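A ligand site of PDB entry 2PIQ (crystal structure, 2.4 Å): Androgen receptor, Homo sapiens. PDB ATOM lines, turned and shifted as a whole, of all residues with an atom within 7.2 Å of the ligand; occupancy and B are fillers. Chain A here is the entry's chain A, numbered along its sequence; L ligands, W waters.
The side-chain amide nitrogen (NE2) of Gln 70 sits at hydrogen-bond distance from the side-chain amide oxygen (OE1) of Gln 234 (3.1 Å).
The backbone carbonyl oxygen of Gln 70 lies close to the indole nitrogen of Trp 73 (3.3 Å).
The backbone NH (N) of Met 226 sits close to the side-chain carboxylate (OE1) of Glu 41, at 3.4 Å.
NH1 of Arg 58 lies within hydrogen-bond range of O of Lys 52, 3.1 Å away.
O of Met 66 lies close to NE2 of Gln 70 (3.4 Å).
The side-chain sulfur (SD) of Met 226 lies close to a nitrogen (N3) of the ligand, 3.6 Å away.
Merely in contact with the ligand: Met 66 (3.3 Å), Ile 230 (3.3 Å), Val 48 (3.7 Å) and Leu 44 (3.9 Å).
Hydrophobic or aromatic side chains that line the ligand: Leu 44, Val 48, Met 66, Met 226 and Ile 230.
Within 4 Å of the ligand: Leu 44, Val 48, Lys 52, Met 66, Gln 70, Met 226 and Ile 230.
Water W1 lies within hydrogen-bond range of an oxygen (O1) of the ligand (3.1 Å), the guanidinium group (NH2) of Arg 58 (3.3 Å) and the side-chain amino group (NZ) of Lys 52 (3.3 Å).
An oxygen (O1) of the ligand lies close to the side-chain amino group of Lys 52 (3.4 Å).
N5 of the ligand sits close to OE1 of Gln 70 (3.3 Å).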
ATOM      1  N   GLU A  41      20.450 -31.783 -22.960  1.00  0.00           N
ATOM      2  CA  GLU A  41      20.803 -31.981 -24.363  1.00  0.00           C
ATOM      3  C   GLU A  41      19.524 -31.988 -25.197  1.00  0.00           C
ATOM      4  O   GLU A  41      19.457 -31.332 -26.233  1.00  0.00           O
ATOM      5  CB  GLU A  41      21.531 -33.321 -24.550  1.00  0.00           C
ATOM      6  CG  GLU A  41      21.919 -33.615 -25.987  1.00  0.00           C
ATOM      7  CD  GLU A  41      23.364 -33.261 -26.286  1.00  0.00           C
ATOM      8  OE1 GLU A  41      23.911 -32.355 -25.633  1.00  0.00           O
ATOM      9  OE2 GLU A  41      23.948 -33.889 -27.201  1.00  0.00           O
ATOM     10  N   LEU A  44      17.845 -28.755 -25.342  1.00  0.00           N
ATOM     11  CA  LEU A  44      18.670 -27.861 -26.134  1.00  0.00           C
ATOM     12  C   LEU A  44      18.232 -27.861 -27.590  1.00  0.00           C
ATOM     13  O   LEU A  44      18.323 -26.844 -28.285  1.00  0.00           O
ATOM     14  CB  LEU A  44      20.143 -28.290 -26.039  1.00  0.00           C
ATOM     15  CG  LEU A  44      21.181 -27.230 -26.418  1.00  0.00           C
ATOM     16  CD1 LEU A  44      21.060 -26.032 -25.468  1.00  0.00           C
ATOM     17  CD2 LEU A  44      22.581 -27.825 -26.344  1.00  0.00           C
ATOM     18  N   VAL A  45      17.756 -29.009 -28.060  1.00  0.00           N
ATOM     19  CA  VAL A  45      17.292 -29.139 -29.440  1.00  0.00           C
ATOM     20  C   VAL A  45      16.044 -28.304 -29.693  1.00  0.00           C
ATOM     21  O   VAL A  45      15.892 -27.700 -30.751  1.00  0.00           O
ATOM     22  CB  VAL A  45      16.995 -30.614 -29.794  1.00  0.00           C
ATOM     23  CG1 VAL A  45      16.349 -30.704 -31.163  1.00  0.00           C
ATOM     24  CG2 VAL A  45      18.275 -31.428 -29.761  1.00  0.00           C
ATOM     25  N   VAL A  48      16.712 -24.372 -29.598  1.00  0.00           N
ATOM     26  CA  VAL A  48      17.278 -23.864 -30.841  1.00  0.00           C
ATOM     27  C   VAL A  48      16.192 -23.648 -31.886  1.00  0.00           C
ATOM     28  O   VAL A  48      16.143 -22.595 -32.523  1.00  0.00           O
ATOM     29  CB  VAL A  48      18.346 -24.842 -31.412  1.00  0.00           C
ATOM     30  CG1 VAL A  48      18.900 -24.312 -32.714  1.00  0.00           C
ATOM     31  CG2 VAL A  48      19.456 -25.034 -30.390  1.00  0.00           C
ATOM     32  N   LYS A  49      15.328 -24.645 -32.050  1.00  0.00           N
ATOM     33  CA  LYS A  49      14.235 -24.548 -33.013  1.00  0.00           C
ATOM     34  C   LYS A  49      13.295 -23.420 -32.611  1.00  0.00           C
ATOM     35  O   LYS A  49      12.842 -22.641 -33.437  1.00  0.00           O
ATOM     36  CB  LYS A  49      13.462 -25.867 -33.063  1.00  0.00           C
ATOM     37  CG  LYS A  49      14.299 -27.071 -33.458  1.00  0.00           C
ATOM     38  CD  LYS A  49      13.474 -28.338 -33.437  1.00  0.00           C
ATOM     39  CE  LYS A  49      14.287 -29.537 -33.919  1.00  0.00           C
ATOM     40  NZ  LYS A  49      13.500 -30.805 -33.897  1.00  0.00           N
ATOM     41  N   LYS A  52      15.010 -19.826 -33.275  1.00  0.00           N
ATOM     42  CA  LYS A  52      15.012 -19.447 -34.692  1.00  0.00           C
ATOM     43  C   LYS A  52      13.610 -19.103 -35.197  1.00  0.00           C
ATOM     44  O   LYS A  52      13.465 -18.386 -36.180  1.00  0.00           O
ATOM     45  CB  LYS A  52      15.597 -20.575 -35.537  1.00  0.00           C
ATOM     46  CG  LYS A  52      16.981 -21.020 -35.096  1.00  0.00           C
ATOM     47  CD  LYS A  52      17.685 -21.838 -36.164  1.00  0.00           C
ATOM     48  CE  LYS A  52      16.945 -23.138 -36.469  1.00  0.00           C
ATOM     49  NZ  LYS A  52      17.541 -23.832 -37.652  1.00  0.00           N
ATOM     50  N   PHE A  57      14.177 -12.907 -34.886  1.00  0.00           N
ATOM     51  CA  PHE A  57      15.408 -13.554 -34.465  1.00  0.00           C
ATOM     52  C   PHE A  57      16.405 -13.638 -35.611  1.00  0.00           C
ATOM     53  O   PHE A  57      17.614 -13.612 -35.405  1.00  0.00           O
ATOM     54  CB  PHE A  57      15.126 -14.964 -33.955  1.00  0.00           C
ATOM     55  CG  PHE A  57      16.323 -15.641 -33.342  1.00  0.00           C
ATOM     56  CD1 PHE A  57      16.754 -15.278 -32.058  1.00  0.00           C
ATOM     57  CD2 PHE A  57      17.033 -16.606 -34.032  1.00  0.00           C
ATOM     58  CE1 PHE A  57      17.880 -15.885 -31.492  1.00  0.00           C
ATOM     59  CE2 PHE A  57      18.151 -17.215 -33.472  1.00  0.00           C
ATOM     60  CZ  PHE A  57      18.567 -16.856 -32.199  1.00  0.00           C
ATOM     61  N   ARG A  58      15.883 -13.740 -36.838  1.00  0.00           N
ATOM     62  CA  ARG A  58      16.737 -13.832 -38.027  1.00  0.00           C
ATOM     63  C   ARG A  58      17.339 -12.478 -38.406  1.00  0.00           C
ATOM     64  O   ARG A  58      17.980 -12.347 -39.446  1.00  0.00           O
ATOM     65  CB  ARG A  58      15.946 -14.413 -39.203  1.00  0.00           C
ATOM     66  CG  ARG A  58      15.269 -15.734 -38.887  1.00  0.00           C
ATOM     67  CD  ARG A  58      14.741 -16.409 -40.149  1.00  0.00           C
ATOM     68  NE  ARG A  58      15.609 -17.509 -40.584  1.00  0.00           N
ATOM     69  CZ  ARG A  58      15.833 -18.611 -39.877  1.00  0.00           C
ATOM     70  NH1 ARG A  58      15.253 -18.765 -38.690  1.00  0.00           N
ATOM     71  NH2 ARG A  58      16.637 -19.559 -40.340  1.00  0.00           N
ATOM     72  N   VAL A  62      24.173 -14.379 -37.888  1.00  0.00           N
ATOM     73  CA  VAL A  62      24.207 -15.820 -37.640  1.00  0.00           C
ATOM     74  C   VAL A  62      25.066 -16.212 -36.439  1.00  0.00           C
ATOM     75  O   VAL A  62      24.702 -17.125 -35.700  1.00  0.00           O
ATOM     76  CB  VAL A  62      24.705 -16.586 -38.890  1.00  0.00           C
ATOM     77  CG1 VAL A  62      26.151 -16.231 -39.189  1.00  0.00           C
ATOM     78  CG2 VAL A  62      24.561 -18.090 -38.671  1.00  0.00           C
ATOM     79  N   ASP A  63      26.186 -15.526 -36.251  1.00  0.00           N
ATOM     80  CA  ASP A  63      27.066 -15.847 -35.118  1.00  0.00           C
ATOM     81  C   ASP A  63      26.464 -15.447 -33.785  1.00  0.00           C
ATOM     82  O   ASP A  63      26.569 -16.194 -32.806  1.00  0.00           O
ATOM     83  CB  ASP A  63      28.433 -15.167 -35.294  1.00  0.00           C
ATOM     84  CG  ASP A  63      29.308 -15.857 -36.325  1.00  0.00           C
ATOM     85  OD1 ASP A  63      29.269 -17.101 -36.397  1.00  0.00           O
ATOM     86  OD2 ASP A  63      30.037 -15.143 -37.050  1.00  0.00           O
ATOM     87  N   GLN A  65      23.391 -15.255 -33.204  1.00  0.00           N
ATOM     88  CA  GLN A  65      22.211 -16.100 -33.008  1.00  0.00           C
ATOM     89  C   GLN A  65      22.599 -17.293 -32.152  1.00  0.00           C
ATOM     90  O   GLN A  65      21.945 -17.595 -31.161  1.00  0.00           O
ATOM     91  CB  GLN A  65      21.679 -16.587 -34.357  1.00  0.00           C
ATOM     92  CG  GLN A  65      20.852 -15.562 -35.114  1.00  0.00           C
ATOM     93  CD  GLN A  65      20.338 -16.103 -36.454  1.00  0.00           C
ATOM     94  OE1 GLN A  65      19.928 -17.250 -36.551  1.00  0.00           O
ATOM     95  NE2 GLN A  65      20.342 -15.245 -37.476  1.00  0.00           N
ATOM     96  N   MET A  66      23.676 -17.971 -32.555  1.00  0.00           N
ATOM     97  CA  MET A  66      24.164 -19.131 -31.827  1.00  0.00           C
ATOM     98  C   MET A  66      24.733 -18.710 -30.473  1.00  0.00           C
ATOM     99  O   MET A  66      24.653 -19.447 -29.488  1.00  0.00           O
ATOM    100  CB  MET A  66      25.258 -19.832 -32.639  1.00  0.00           C
ATOM    101  CG  MET A  66      26.002 -20.921 -31.868  1.00  0.00           C
ATOM    102  SD  MET A  66      27.431 -21.559 -32.774  1.00  0.00           S
ATOM    103  CE  MET A  66      26.844 -23.208 -33.228  1.00  0.00           C
ATOM    104  N   ALA A  67      25.308 -17.507 -30.444  1.00  0.00           N
ATOM    105  CA  ALA A  67      25.897 -16.961 -29.225  1.00  0.00           C
ATOM    106  C   ALA A  67      24.882 -16.803 -28.113  1.00  0.00           C
ATOM    107  O   ALA A  67      25.002 -17.435 -27.071  1.00  0.00           O
ATOM    108  CB  ALA A  67      26.548 -15.608 -29.533  1.00  0.00           C
ATOM    109  N   VAL A  68      23.880 -15.971 -28.336  1.00  0.00           N
ATOM    110  CA  VAL A  68      22.834 -15.725 -27.328  1.00  0.00           C
ATOM    111  C   VAL A  68      22.203 -17.019 -26.827  1.00  0.00           C
ATOM    112  O   VAL A  68      21.774 -17.090 -25.681  1.00  0.00           O
ATOM    113  CB  VAL A  68      21.718 -14.814 -27.901  1.00  0.00           C
ATOM    114  CG1 VAL A  68      22.315 -13.476 -28.301  1.00  0.00           C
ATOM    115  CG2 VAL A  68      21.055 -15.480 -29.086  1.00  0.00           C
ATOM    116  N   ILE A  69      22.139 -18.030 -27.688  1.00  0.00           N
ATOM    117  CA  ILE A  69      21.562 -19.315 -27.313  1.00  0.00           C
ATOM    118  C   ILE A  69      22.494 -20.086 -26.383  1.00  0.00           C
ATOM    119  O   ILE A  69      22.043 -20.704 -25.414  1.00  0.00           O
ATOM    120  CB  ILE A  69      21.265 -20.183 -28.553  1.00  0.00           C
ATOM    121  CG1 ILE A  69      20.126 -19.558 -29.363  1.00  0.00           C
ATOM    122  CG2 ILE A  69      20.905 -21.592 -28.142  1.00  0.00           C
ATOM    123  CD1 ILE A  69      19.727 -20.371 -30.568  1.00  0.00           C
ATOM    124  N   GLN A  70      23.784 -20.062 -26.678  1.00  0.00           N
ATOM    125  CA  GLN A  70      24.781 -20.749 -25.879  1.00  0.00           C
ATOM    126  C   GLN A  70      25.050 -20.096 -24.534  1.00  0.00           C
ATOM    127  O   GLN A  70      25.688 -20.686 -23.657  1.00  0.00           O
ATOM    128  CB  GLN A  70      26.082 -20.885 -26.667  1.00  0.00           C
ATOM    129  CG  GLN A  70      26.062 -21.985 -27.713  1.00  0.00           C
ATOM    130  CD  GLN A  70      27.192 -21.849 -28.730  1.00  0.00           C
ATOM    131  OE1 GLN A  70      27.510 -22.802 -29.441  1.00  0.00           O
ATOM    132  NE2 GLN A  70      27.775 -20.660 -28.810  1.00  0.00           N
ATOM    133  N   TYR A  71      24.571 -18.861 -24.359  1.00  0.00           N
ATOM    134  CA  TYR A  71      24.792 -18.143 -23.106  1.00  0.00           C
ATOM    135  C   TYR A  71      23.565 -18.103 -22.218  1.00  0.00           C
ATOM    136  O   TYR A  71      23.688 -18.045 -20.986  1.00  0.00           O
ATOM    137  CB  TYR A  71      25.247 -16.701 -23.383  1.00  0.00           C
ATOM    138  CG  TYR A  71      26.545 -16.570 -24.165  1.00  0.00           C
ATOM    139  CD1 TYR A  71      27.644 -17.349 -23.849  1.00  0.00           C
ATOM    140  CD2 TYR A  71      26.659 -15.635 -25.189  1.00  0.00           C
ATOM    141  CE1 TYR A  71      28.854 -17.200 -24.553  1.00  0.00           C
ATOM    142  CE2 TYR A  71      27.870 -15.486 -25.893  1.00  0.00           C
ATOM    143  CZ  TYR A  71      28.947 -16.261 -25.567  1.00  0.00           C
ATOM    144  OH  TYR A  71      30.130 -16.123 -26.247  1.00  0.00           O
ATOM    145  N   TRP A  73      20.830 -20.422 -22.573  1.00  0.00           N
ATOM    146  CA  TRP A  73      20.073 -21.672 -22.598  1.00  0.00           C
ATOM    147  C   TRP A  73      19.757 -22.130 -21.178  1.00  0.00           C
ATOM    148  O   TRP A  73      18.744 -22.798 -20.937  1.00  0.00           O
ATOM    149  CB  TRP A  73      20.850 -22.771 -23.318  1.00  0.00           C
ATOM    150  CG  TRP A  73      22.143 -23.168 -22.651  1.00  0.00           C
ATOM    151  CD1 TRP A  73      23.378 -22.685 -22.928  1.00  0.00           C
ATOM    152  CD2 TRP A  73      22.298 -24.102 -21.579  1.00  0.00           C
ATOM    153  NE1 TRP A  73      24.300 -23.262 -22.096  1.00  0.00           N
ATOM    154  CE2 TRP A  73      23.667 -24.139 -21.261  1.00  0.00           C
ATOM    155  CE3 TRP A  73      21.409 -24.911 -20.864  1.00  0.00           C
ATOM    156  CZ2 TRP A  73      24.179 -24.960 -20.246  1.00  0.00           C
ATOM    157  CZ3 TRP A  73      21.913 -25.734 -19.854  1.00  0.00           C
ATOM    158  CH2 TRP A  73      23.296 -25.756 -19.560  1.00  0.00           C
ATOM    159  N   MET A 226      26.913 -32.229 -27.120  1.00  0.00           N
ATOM    160  CA  MET A 226      26.680 -30.789 -27.136  1.00  0.00           C
ATOM    161  C   MET A 226      26.724 -30.131 -25.762  1.00  0.00           C
ATOM    162  O   MET A 226      27.111 -28.979 -25.636  1.00  0.00           O
ATOM    163  CB  MET A 226      25.349 -30.480 -27.828  1.00  0.00           C
ATOM    164  CG  MET A 226      25.485 -30.371 -29.341  1.00  0.00           C
ATOM    165  SD  MET A 226      23.925 -30.541 -30.224  1.00  0.00           S
ATOM    166  CE  MET A 226      23.982 -32.281 -30.680  1.00  0.00           C
ATOM    167  N   MET A 227      26.319 -30.868 -24.733  1.00  0.00           N
ATOM    168  CA  MET A 227      26.331 -30.347 -23.375  1.00  0.00           C
ATOM    169  C   MET A 227      27.773 -30.139 -22.908  1.00  0.00           C
ATOM    170  O   MET A 227      28.121 -29.069 -22.396  1.00  0.00           O
ATOM    171  CB  MET A 227      25.624 -31.309 -22.415  1.00  0.00           C
ATOM    172  CG  MET A 227      24.107 -31.275 -22.482  1.00  0.00           C
ATOM    173  SD  MET A 227      23.390 -29.776 -21.760  1.00  0.00           S
ATOM    174  CE  MET A 227      22.902 -28.900 -23.218  1.00  0.00           C
ATOM    175  N   ILE A 230      29.392 -27.038 -24.824  1.00  0.00           N
ATOM    176  CA  ILE A 230      28.852 -25.737 -24.434  1.00  0.00           C
ATOM    177  C   ILE A 230      29.286 -25.351 -23.023  1.00  0.00           C
ATOM    178  O   ILE A 230      29.587 -24.190 -22.749  1.00  0.00           O
ATOM    179  CB  ILE A 230      27.303 -25.730 -24.500  1.00  0.00           C
ATOM    180  CG1 ILE A 230      26.844 -25.598 -25.953  1.00  0.00           C
ATOM    181  CG2 ILE A 230      26.740 -24.584 -23.655  1.00  0.00           C
ATOM    182  CD1 ILE A 230      25.340 -25.670 -26.141  1.00  0.00           C
ATOM    183  N   GLN A 234      31.586 -22.380 -23.735  1.00  0.00           N
ATOM    184  CA  GLN A 234      30.776 -21.172 -23.583  1.00  0.00           C
ATOM    185  C   GLN A 234      30.647 -20.757 -22.124  1.00  0.00           C
ATOM    186  O   GLN A 234      30.970 -19.631 -21.766  1.00  0.00           O
ATOM    187  CB  GLN A 234      29.396 -21.393 -24.198  1.00  0.00           C
ATOM    188  CG  GLN A 234      29.428 -21.987 -25.591  1.00  0.00           C
ATOM    189  CD  GLN A 234      30.145 -21.105 -26.593  1.00  0.00           C
ATOM    190  OE1 GLN A 234      30.521 -21.559 -27.674  1.00  0.00           O
ATOM    191  NE2 GLN A 234      30.320 -19.827 -26.254  1.00  0.00           N
HETATM  192  C1  LIG L   1      21.645 -27.165 -34.754  1.00  0.00           C
HETATM  193  C2  LIG L   1      22.370 -27.473 -33.434  1.00  0.00           C
HETATM  194  C3  LIG L   1      21.451 -28.275 -32.511  1.00  0.00           C
HETATM  195  C4  LIG L   1      23.654 -28.271 -33.721  1.00  0.00           C
HETATM  196  N1  LIG L   1      22.738 -26.182 -32.779  1.00  0.00           N
HETATM  197  N2  LIG L   1      22.474 -25.080 -33.261  1.00  0.00           N
HETATM  198  C5  LIG L   1      23.365 -26.086 -31.607  1.00  0.00           C
HETATM  199  N3  LIG L   1      23.829 -26.974 -30.710  1.00  0.00           N
HETATM  200  C6  LIG L   1      24.420 -26.564 -29.604  1.00  0.00           C
HETATM  201  N4  LIG L   1      24.573 -25.273 -29.341  1.00  0.00           N
HETATM  202  C7  LIG L   1      24.119 -24.329 -30.183  1.00  0.00           C
HETATM  203  N5  LIG L   1      24.279 -23.037 -29.915  1.00  0.00           N
HETATM  204  C8  LIG L   1      23.492 -24.722 -31.366  1.00  0.00           C
HETATM  205  C9  LIG L   1      22.919 -24.104 -32.458  1.00  0.00           C
HETATM  206  C10 LIG L   1      22.772 -22.599 -32.713  1.00  0.00           C
HETATM  207  C11 LIG L   1      22.770 -22.305 -34.200  1.00  0.00           C
HETATM  208  C12 LIG L   1      21.603 -22.431 -34.960  1.00  0.00           C
HETATM  209  C13 LIG L   1      23.951 -21.890 -34.827  1.00  0.00           C
HETATM  210  C14 LIG L   1      23.957 -21.601 -36.186  1.00  0.00           C
HETATM  211  C15 LIG L   1      22.779 -21.714 -36.936  1.00  0.00           C
HETATM  212  C16 LIG L   1      21.609 -22.142 -36.320  1.00  0.00           C
HETATM  213  O1  LIG L   1      20.471 -22.268 -37.051  1.00  0.00           O
HETATM  214  O   HOH W   1      19.049 -21.652 -39.678  1.00  0.00           O
